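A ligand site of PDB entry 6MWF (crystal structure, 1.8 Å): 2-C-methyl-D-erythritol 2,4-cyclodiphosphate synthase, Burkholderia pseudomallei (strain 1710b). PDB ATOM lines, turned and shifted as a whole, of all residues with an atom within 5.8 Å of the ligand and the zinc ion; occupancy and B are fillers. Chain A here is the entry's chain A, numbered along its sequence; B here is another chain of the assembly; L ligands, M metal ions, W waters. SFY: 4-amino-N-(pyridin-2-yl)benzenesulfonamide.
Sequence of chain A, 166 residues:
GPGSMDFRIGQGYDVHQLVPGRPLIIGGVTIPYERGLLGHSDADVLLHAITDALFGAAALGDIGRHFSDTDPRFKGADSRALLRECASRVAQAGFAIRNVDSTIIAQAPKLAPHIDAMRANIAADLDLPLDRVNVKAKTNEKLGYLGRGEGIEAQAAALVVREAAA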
ATOM      1  N   TYR A  13       3.326  -5.946  17.996  1.00  0.00           N
ATOM      2  CA  TYR A  13       4.109  -6.812  17.135  1.00  0.00           C
ATOM      3  C   TYR A  13       5.516  -6.246  17.060  1.00  0.00           C
ATOM      4  O   TYR A  13       5.675  -5.029  16.968  1.00  0.00           O
ATOM      5  CB  TYR A  13       3.503  -6.875  15.717  1.00  0.00           C
ATOM      6  CG  TYR A  13       4.431  -7.467  14.667  1.00  0.00           C
ATOM      7  CD1 TYR A  13       4.519  -8.837  14.521  1.00  0.00           C
ATOM      8  CD2 TYR A  13       5.221  -6.669  13.860  1.00  0.00           C
ATOM      9  CE1 TYR A  13       5.356  -9.411  13.583  1.00  0.00           C
ATOM     10  CE2 TYR A  13       6.078  -7.235  12.916  1.00  0.00           C
ATOM     11  CZ  TYR A  13       6.130  -8.601  12.790  1.00  0.00           C
ATOM     12  OH  TYR A  13       6.967  -9.175  11.852  1.00  0.00           O
ATOM     13  N   ASP A  14       6.531  -7.110  17.049  1.00  0.00           N
ATOM     14  CA  ASP A  14       7.856  -6.603  16.736  1.00  0.00           C
ATOM     15  C   ASP A  14       8.689  -7.740  16.150  1.00  0.00           C
ATOM     16  O   ASP A  14       8.433  -8.915  16.397  1.00  0.00           O
ATOM     17  CB  ASP A  14       8.530  -6.011  17.974  1.00  0.00           C
ATOM     18  CG  ASP A  14       9.731  -5.119  17.626  1.00  0.00           C
ATOM     19  OD1 ASP A  14       9.830  -4.649  16.470  1.00  0.00           O
ATOM     20  OD2 ASP A  14      10.590  -4.884  18.498  1.00  0.00           O
ATOM     21  N   VAL A  15       9.723  -7.362  15.397  1.00  0.00           N
ATOM     22  CA  VAL A  15      10.671  -8.331  14.859  1.00  0.00           C
ATOM     23  C   VAL A  15      12.032  -7.660  14.801  1.00  0.00           C
ATOM     24  O   VAL A  15      12.133  -6.459  14.555  1.00  0.00           O
ATOM     25  CB  VAL A  15      10.227  -8.842  13.468  1.00  0.00           C
ATOM     26  CG1 VAL A  15      10.247  -7.729  12.424  1.00  0.00           C
ATOM     27  CG2 VAL A  15      11.095 -10.034  13.032  1.00  0.00           C
ATOM     28  N   HIS A  16      13.094  -8.433  15.051  1.00  0.00           N
ATOM     29  CA  HIS A  16      14.456  -7.971  14.859  1.00  0.00           C
ATOM     30  C   HIS A  16      15.285  -9.076  14.225  1.00  0.00           C
ATOM     31  O   HIS A  16      15.084 -10.258  14.491  1.00  0.00           O
ATOM     32  CB  HIS A  16      15.119  -7.538  16.196  1.00  0.00           C
ATOM     33  CG  HIS A  16      14.610  -6.228  16.723  1.00  0.00           C
ATOM     34  ND1 HIS A  16      15.233  -5.031  16.455  1.00  0.00           N
ATOM     35  CD2 HIS A  16      13.535  -5.934  17.495  1.00  0.00           C
ATOM     36  CE1 HIS A  16      14.558  -4.049  17.046  1.00  0.00           C
ATOM     37  NE2 HIS A  16      13.528  -4.572  17.676  1.00  0.00           N
ATOM     38  N   LEU A  38      19.500  -7.286  16.398  1.00  0.00           N
ATOM     39  CA  LEU A  38      20.009  -6.045  15.833  1.00  0.00           C
ATOM     40  C   LEU A  38      18.964  -4.935  15.959  1.00  0.00           C
ATOM     41  O   LEU A  38      17.834  -5.082  15.496  1.00  0.00           O
ATOM     42  CB  LEU A  38      20.367  -6.231  14.355  1.00  0.00           C
ATOM     43  CG  LEU A  38      20.861  -5.023  13.590  1.00  0.00           C
ATOM     44  CD1 LEU A  38      22.247  -4.641  14.093  1.00  0.00           C
ATOM     45  CD2 LEU A  38      20.866  -5.348  12.105  1.00  0.00           C
ATOM     46  N   GLY A  39      19.382  -3.807  16.534  1.00  0.00           N
ATOM     47  CA  GLY A  39      18.495  -2.672  16.635  1.00  0.00           C
ATOM     48  C   GLY A  39      19.241  -1.487  17.177  1.00  0.00           C
ATOM     49  O   GLY A  39      20.406  -1.591  17.593  1.00  0.00           O
ATOM     50  N   HIS A  40      18.574  -0.336  17.138  1.00  0.00           N
ATOM     51  CA  HIS A  40      19.159   0.896  17.676  1.00  0.00           C
ATOM     52  C   HIS A  40      19.308   0.803  19.197  1.00  0.00           C
ATOM     53  O   HIS A  40      20.355   1.146  19.752  1.00  0.00           O
ATOM     54  CB  HIS A  40      18.277   2.082  17.276  1.00  0.00           C
ATOM     55  CG  HIS A  40      18.797   3.408  17.710  1.00  0.00           C
ATOM     56  ND1 HIS A  40      20.005   3.902  17.281  1.00  0.00           N
ATOM     57  CD2 HIS A  40      18.259   4.360  18.517  1.00  0.00           C
ATOM     58  CE1 HIS A  40      20.203   5.093  17.829  1.00  0.00           C
ATOM     59  NE2 HIS A  40      19.159   5.390  18.577  1.00  0.00           N
ATOM     60  N   SER A  41      18.259   0.324  19.873  1.00  0.00           N
ATOM     61  CA  SER A  41      18.270   0.088  21.304  1.00  0.00           C
ATOM     62  C   SER A  41      18.920  -1.262  21.588  1.00  0.00           C
ATOM     63  O   SER A  41      19.601  -1.809  20.715  1.00  0.00           O
ATOM     64  CB  SER A  41      16.839   0.118  21.861  1.00  0.00           C
ATOM     65  OG  SER A  41      16.100  -1.061  21.506  1.00  0.00           O
ATOM     66  N   ASP A  42      18.702  -1.822  22.780  1.00  0.00           N
ATOM     67  CA  ASP A  42      19.187  -3.175  22.987  1.00  0.00           C
ATOM     68  C   ASP A  42      18.393  -4.204  22.195  1.00  0.00           C
ATOM     69  O   ASP A  42      18.688  -5.406  22.277  1.00  0.00           O
ATOM     70  CB  ASP A  42      19.184  -3.524  24.485  1.00  0.00           C
ATOM     71  CG  ASP A  42      17.791  -3.611  25.094  1.00  0.00           C
ATOM     72  OD1 ASP A  42      16.768  -3.584  24.366  1.00  0.00           O
ATOM     73  OD2 ASP A  42      17.731  -3.705  26.338  1.00  0.00           O
ATOM     74  N   ALA A  43      17.392  -3.761  21.425  1.00  0.00           N
ATOM     75  CA  ALA A  43      16.682  -4.589  20.453  1.00  0.00           C
ATOM     76  C   ALA A  43      15.827  -5.679  21.099  1.00  0.00           C
ATOM     77  O   ALA A  43      15.597  -6.738  20.495  1.00  0.00           O
ATOM     78  CB  ALA A  43      17.636  -5.196  19.418  1.00  0.00           C
ATOM     79  N   ASP A  44      15.331  -5.435  22.301  1.00  0.00           N
ATOM     80  CA  ASP A  44      14.511  -6.404  23.019  1.00  0.00           C
ATOM     81  C   ASP A  44      13.128  -6.504  22.390  1.00  0.00           C
ATOM     82  O   ASP A  44      12.204  -5.743  22.711  1.00  0.00           O
ATOM     83  CB  ASP A  44      14.407  -6.022  24.499  1.00  0.00           C
ATOM     84  CG  ASP A  44      13.881  -7.161  25.358  1.00  0.00           C
ATOM     85  OD1 ASP A  44      12.980  -7.923  24.909  1.00  0.00           O
ATOM     86  OD2 ASP A  44      14.371  -7.281  26.501  1.00  0.00           O
ATOM     87  N   VAL A  45      12.993  -7.478  21.480  1.00  0.00           N
ATOM     88  CA  VAL A  45      11.798  -7.578  20.635  1.00  0.00           C
ATOM     89  C   VAL A  45      10.550  -7.847  21.487  1.00  0.00           C
ATOM     90  O   VAL A  45       9.441  -7.381  21.161  1.00  0.00           O
ATOM     91  CB  VAL A  45      12.052  -8.668  19.574  1.00  0.00           C
ATOM     92  CG1 VAL A  45      12.299 -10.027  20.220  1.00  0.00           C
ATOM     93  CG2 VAL A  45      10.919  -8.753  18.553  1.00  0.00           C
ATOM     94  N   HIS A  48       9.533  -4.635  23.324  1.00  0.00           N
ATOM     95  CA  HIS A  48       8.997  -3.666  22.372  1.00  0.00           C
ATOM     96  C   HIS A  48       7.557  -4.009  21.998  1.00  0.00           C
ATOM     97  O   HIS A  48       6.697  -3.117  21.885  1.00  0.00           O
ATOM     98  CB  HIS A  48       9.866  -3.587  21.110  1.00  0.00           C
ATOM     99  CG  HIS A  48      11.255  -3.079  21.373  1.00  0.00           C
ATOM    100  ND1 HIS A  48      12.240  -3.061  20.424  1.00  0.00           N
ATOM    101  CD2 HIS A  48      11.805  -2.543  22.499  1.00  0.00           C
ATOM    102  CE1 HIS A  48      13.354  -2.571  20.935  1.00  0.00           C
ATOM    103  NE2 HIS A  48      13.118  -2.250  22.197  1.00  0.00           N
ATOM    104  N   ASP A  52       4.346  -1.590  22.716  1.00  0.00           N
ATOM    105  CA  ASP A  52       3.402  -1.167  21.680  1.00  0.00           C
ATOM    106  C   ASP A  52       1.968  -1.505  22.067  1.00  0.00           C
ATOM    107  O   ASP A  52       1.045  -0.715  21.816  1.00  0.00           O
ATOM    108  CB  ASP A  52       3.766  -1.812  20.336  1.00  0.00           C
ATOM    109  CG  ASP A  52       4.293  -0.815  19.320  1.00  0.00           C
ATOM    110  OD1 ASP A  52       4.606   0.319  19.716  1.00  0.00           O
ATOM    111  OD2 ASP A  52       4.408  -1.141  18.100  1.00  0.00           O
ATOM    112  N   ILE A  63       5.629   2.891  19.946  1.00  0.00           N
ATOM    113  CA  ILE A  63       6.961   3.060  20.504  1.00  0.00           C
ATOM    114  C   ILE A  63       7.789   4.012  19.650  1.00  0.00           C
ATOM    115  O   ILE A  63       8.588   4.794  20.183  1.00  0.00           O
ATOM    116  CB  ILE A  63       7.593   1.656  20.680  1.00  0.00           C
ATOM    117  CG1 ILE A  63       8.854   1.729  21.524  1.00  0.00           C
ATOM    118  CG2 ILE A  63       7.886   1.017  19.330  1.00  0.00           C
ATOM    119  CD1 ILE A  63       9.430   0.339  21.856  1.00  0.00           C
ATOM    120  N   GLY A  64       7.581   4.016  18.334  1.00  0.00           N
ATOM    121  CA  GLY A  64       8.275   4.972  17.489  1.00  0.00           C
ATOM    122  C   GLY A  64       7.923   6.416  17.809  1.00  0.00           C
ATOM    123  O   GLY A  64       8.769   7.300  17.738  1.00  0.00           O
ATOM    124  N   PHE A  67       9.645   6.989  21.569  1.00  0.00           N
ATOM    125  CA  PHE A  67      11.081   6.771  21.703  1.00  0.00           C
ATOM    126  C   PHE A  67      11.663   6.517  20.303  1.00  0.00           C
ATOM    127  O   PHE A  67      11.890   5.362  19.906  1.00  0.00           O
ATOM    128  CB  PHE A  67      11.407   5.603  22.628  1.00  0.00           C
ATOM    129  CG  PHE A  67      10.595   5.524  23.898  1.00  0.00           C
ATOM    130  CD1 PHE A  67      10.776   6.437  24.940  1.00  0.00           C
ATOM    131  CD2 PHE A  67       9.738   4.443  24.109  1.00  0.00           C
ATOM    132  CE1 PHE A  67      10.066   6.311  26.123  1.00  0.00           C
ATOM    133  CE2 PHE A  67       9.012   4.315  25.306  1.00  0.00           C
ATOM    134  CZ  PHE A  67       9.174   5.246  26.310  1.00  0.00           C
ATOM    135  N   SER A  68      11.944   7.586  19.564  1.00  0.00           N
ATOM    136  CA  SER A  68      12.335   7.442  18.163  1.00  0.00           C
ATOM    137  C   SER A  68      13.630   6.644  18.012  1.00  0.00           C
ATOM    138  O   SER A  68      14.603   6.893  18.738  1.00  0.00           O
ATOM    139  CB  SER A  68      12.489   8.820  17.522  1.00  0.00           C
ATOM    140  OG  SER A  68      13.606   9.499  18.072  1.00  0.00           O
ATOM    141  N   ASP A  69      13.639   5.704  17.061  1.00  0.00           N
ATOM    142  CA  ASP A  69      14.850   4.945  16.762  1.00  0.00           C
ATOM    143  C   ASP A  69      15.904   5.787  16.065  1.00  0.00           C
ATOM    144  O   ASP A  69      17.016   5.291  15.830  1.00  0.00           O
ATOM    145  CB  ASP A  69      14.519   3.723  15.901  1.00  0.00           C
ATOM    146  N   THR A  70      15.591   7.027  15.709  1.00  0.00           N
ATOM    147  CA  THR A  70      16.587   7.939  15.172  1.00  0.00           C
ATOM    148  C   THR A  70      17.343   8.680  16.256  1.00  0.00           C
ATOM    149  O   THR A  70      18.412   9.230  15.979  1.00  0.00           O
ATOM    150  CB  THR A  70      15.912   8.948  14.227  1.00  0.00           C
ATOM    151  N   PHE A  74      18.777   7.014  22.641  1.00  0.00           N
ATOM    152  CA  PHE A  74      18.285   5.665  22.801  1.00  0.00           C
ATOM    153  C   PHE A  74      19.200   4.625  22.184  1.00  0.00           C
ATOM    154  O   PHE A  74      18.832   3.453  22.130  1.00  0.00           O
ATOM    155  CB  PHE A  74      16.872   5.548  22.196  1.00  0.00           C
ATOM    156  CG  PHE A  74      15.856   6.427  22.863  1.00  0.00           C
ATOM    157  CD1 PHE A  74      15.183   7.410  22.142  1.00  0.00           C
ATOM    158  CD2 PHE A  74      15.574   6.293  24.211  1.00  0.00           C
ATOM    159  CE1 PHE A  74      14.255   8.224  22.753  1.00  0.00           C
ATOM    160  CE2 PHE A  74      14.651   7.113  24.827  1.00  0.00           C
ATOM    161  CZ  PHE A  74      13.993   8.083  24.093  1.00  0.00           C
ATOM    162  N   ALA A  77      19.745   1.633  24.280  1.00  0.00           N
ATOM    163  CA  ALA A  77      18.863   1.820  25.426  1.00  0.00           C
ATOM    164  C   ALA A  77      18.405   0.506  26.016  1.00  0.00           C
ATOM    165  O   ALA A  77      18.106  -0.452  25.303  1.00  0.00           O
ATOM    166  CB  ALA A  77      17.639   2.653  25.029  1.00  0.00           C
ATOM    167  N   SER A  79      15.715  -1.638  27.211  1.00  0.00           N
ATOM    168  CA  SER A  79      14.300  -1.609  26.891  1.00  0.00           C
ATOM    169  C   SER A  79      13.410  -1.834  28.113  1.00  0.00           C
ATOM    170  O   SER A  79      12.200  -1.594  28.007  1.00  0.00           O
ATOM    171  CB  SER A  79      13.983  -2.642  25.813  1.00  0.00           C
ATOM    172  OG  SER A  79      14.591  -2.236  24.578  1.00  0.00           O
ATOM    173  N   LEU A  82      12.667   1.671  28.994  1.00  0.00           N
ATOM    174  CA  LEU A  82      11.647   2.168  28.079  1.00  0.00           C
ATOM    175  C   LEU A  82      10.270   1.627  28.451  1.00  0.00           C
ATOM    176  O   LEU A  82       9.279   2.354  28.413  1.00  0.00           O
ATOM    177  CB  LEU A  82      11.992   1.786  26.643  1.00  0.00           C
ATOM    178  CG  LEU A  82      13.312   2.337  26.072  1.00  0.00           C
ATOM    179  CD1 LEU A  82      13.482   1.875  24.634  1.00  0.00           C
ATOM    180  CD2 LEU A  82      13.358   3.855  26.175  1.00  0.00           C
ATOM    181  N   LYS B 138       5.039   0.111  11.682  1.00  0.00           N
ATOM    182  CA  LYS B 138       6.445  -0.251  11.747  1.00  0.00           C
ATOM    183  C   LYS B 138       6.864  -0.973  10.481  1.00  0.00           C
ATOM    184  O   LYS B 138       6.062  -1.331   9.636  1.00  0.00           O
ATOM    185  CB  LYS B 138       6.749  -1.117  12.949  1.00  0.00           C
ATOM    186  CG  LYS B 138       6.123  -2.506  12.905  1.00  0.00           C
ATOM    187  CD  LYS B 138       5.727  -2.945  14.303  1.00  0.00           C
ATOM    188  CE  LYS B 138       6.478  -2.169  15.385  1.00  0.00           C
ATOM    189  NZ  LYS B 138       7.922  -2.552  15.463  1.00  0.00           N
ATOM    190  N   GLU B 141      11.931  -4.827   9.348  1.00  0.00           N
ATOM    191  CA  GLU B 141      13.382  -4.988   9.475  1.00  0.00           C
ATOM    192  C   GLU B 141      13.957  -5.750   8.288  1.00  0.00           C
ATOM    193  O   GLU B 141      14.878  -6.565   8.421  1.00  0.00           O
ATOM    194  CB  GLU B 141      13.747  -5.679  10.803  1.00  0.00           C
ATOM    195  CG  GLU B 141      13.462  -4.838  12.026  1.00  0.00           C
ATOM    196  CD  GLU B 141      14.336  -3.613  12.121  1.00  0.00           C
ATOM    197  OE1 GLU B 141      15.577  -3.717  11.976  1.00  0.00           O
ATOM    198  OE2 GLU B 141      13.779  -2.517  12.326  1.00  0.00           O
HETATM  199  OAB SFY L   1      16.006  -1.165  18.751  1.00  0.00           O
HETATM  200  SAQ SFY L   1      14.893  -0.344  18.009  1.00  0.00           S
HETATM  201  OAC SFY L   1      15.168   0.267  16.575  1.00  0.00           O
HETATM  202  CAP SFY L   1      14.501   1.003  19.118  1.00  0.00           C
HETATM  203  CAJ SFY L   1      13.641   0.821  20.173  1.00  0.00           C
HETATM  204  CAH SFY L   1      13.391   1.872  21.028  1.00  0.00           C
HETATM  205  CAN SFY L   1      14.042   3.104  20.848  1.00  0.00           C
HETATM  206  NAA SFY L   1      13.828   4.150  21.683  1.00  0.00           N
HETATM  207  CAI SFY L   1      14.940   3.237  19.787  1.00  0.00           C
HETATM  208  CAK SFY L   1      15.178   2.193  18.933  1.00  0.00           C
HETATM  209  NAM SFY L   1      13.437  -1.245  18.007  1.00  0.00           N
HETATM  210  CAO SFY L   1      12.206  -0.798  17.560  1.00  0.00           C
HETATM  211  CAG SFY L   1      12.003   0.478  17.055  1.00  0.00           C
HETATM  212  CAE SFY L   1      10.736   0.807  16.646  1.00  0.00           C
HETATM  213  CAD SFY L   1       9.713  -0.125  16.748  1.00  0.00           C
HETATM  214  CAF SFY L   1      10.012  -1.366  17.279  1.00  0.00           C
HETATM  215  NAL SFY L   1      11.244  -1.693  17.660  1.00  0.00           N
HETATM  216 ZN    ZN M   1      11.998  -3.508  18.491  1.00  0.00          ZN
HETATM  217  O   HOH W   1      15.874  -1.873  14.268  1.00  0.00           O
HETATM  218  O   HOH W   2      11.165   3.984  15.607  1.00  0.00           O
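Water W1 lies within hydrogen-bond range of OE2 of Glu 141 of chain B and OAC of the ligand.
The zinc ion is bound by OD2 of Asp 14.
ND1 of His 48 binds the zinc ion, 2.0 Å away.
NE2 of His 16 is bound to the zinc ion (2.0 Å).
The zinc ion is bound by NAL of the ligand (2.1 Å).
Slightly farther from the zinc ion lies NAM of the ligand (2.7 Å).
The side-chain hydroxyl (OG) of Ser 41 sits close to a ring nitrogen (NE2) of His 48, 3.3 Å away.
A ring nitrogen (NE2) of His 48 sits at hydrogen-bond distance from the side-chain hydroxyl (OG) of Ser 79.
The side-chain carboxylate (OD1) of Asp 14 lies within salt-bridge range of the side-chain amino group (NZ) of Lys 138 of chain B.
The side-chain hydroxyl (OG) of Ser 41 sits close to the backbone NH (N) of Ala 43 (3.0 Å).
The backbone carbonyl oxygen (O) of Leu 38 sits at hydrogen-bond distance from a ring nitrogen (ND1) of His 16, 2.8 Å away.
The backbone NH (N) of Ile 63 is in hydrogen-bond range of the side-chain carboxylate (OD1) of Asp 52, at 2.8 Å.
A ring nitrogen (NE2) of His 40 lies close to the backbone carbonyl oxygen (O) of Asp 69, 3.5 Å away.
The side-chain hydroxyl (OG) of Ser 41 sits at hydrogen-bond distance from an oxygen (OAB) of the ligand.
An oxygen (OAB) of the ligand is in hydrogen-bond range of the backbone NH (N) of Ser 41 (2.9 Å).
N of His 40 is in hydrogen-bond range of OAB of the ligand.
NAA of the ligand sits at hydrogen-bond distance from O of Phe 67 (2.9 Å).
Gly 39 touches the ligand.
Ala 43 touches the ligand.
Ile 63 touches the ligand.
Ser 68 touches the ligand.
Asp 69 touches the ligand.
CG of Phe 74 touches NAA of the ligand, at 3.3 Å.
Leu 82 touches the ligand (CD1 to CAH, 3.6 Å).
Lys 138 of chain B touches the ligand (NZ to CAF, 3.0 Å).
Hydrophobic or aromatic side chains within 4 Å of the ligand: His 16, His 40, His 48, Ile 63, Phe 67, Phe 74 and Leu 82.
Within 4 Å of the ligand: Asp 14, His 16, Gly 39, His 40, Ser 41, Ala 43, His 48, Ile 63, Phe 67, Ser 68, Asp 69, Phe 74, Leu 82 and Lys 138 of chain B.
Three residues have an atom within 4 Å of the zinc ion: Asp 14, His 16 and His 48.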
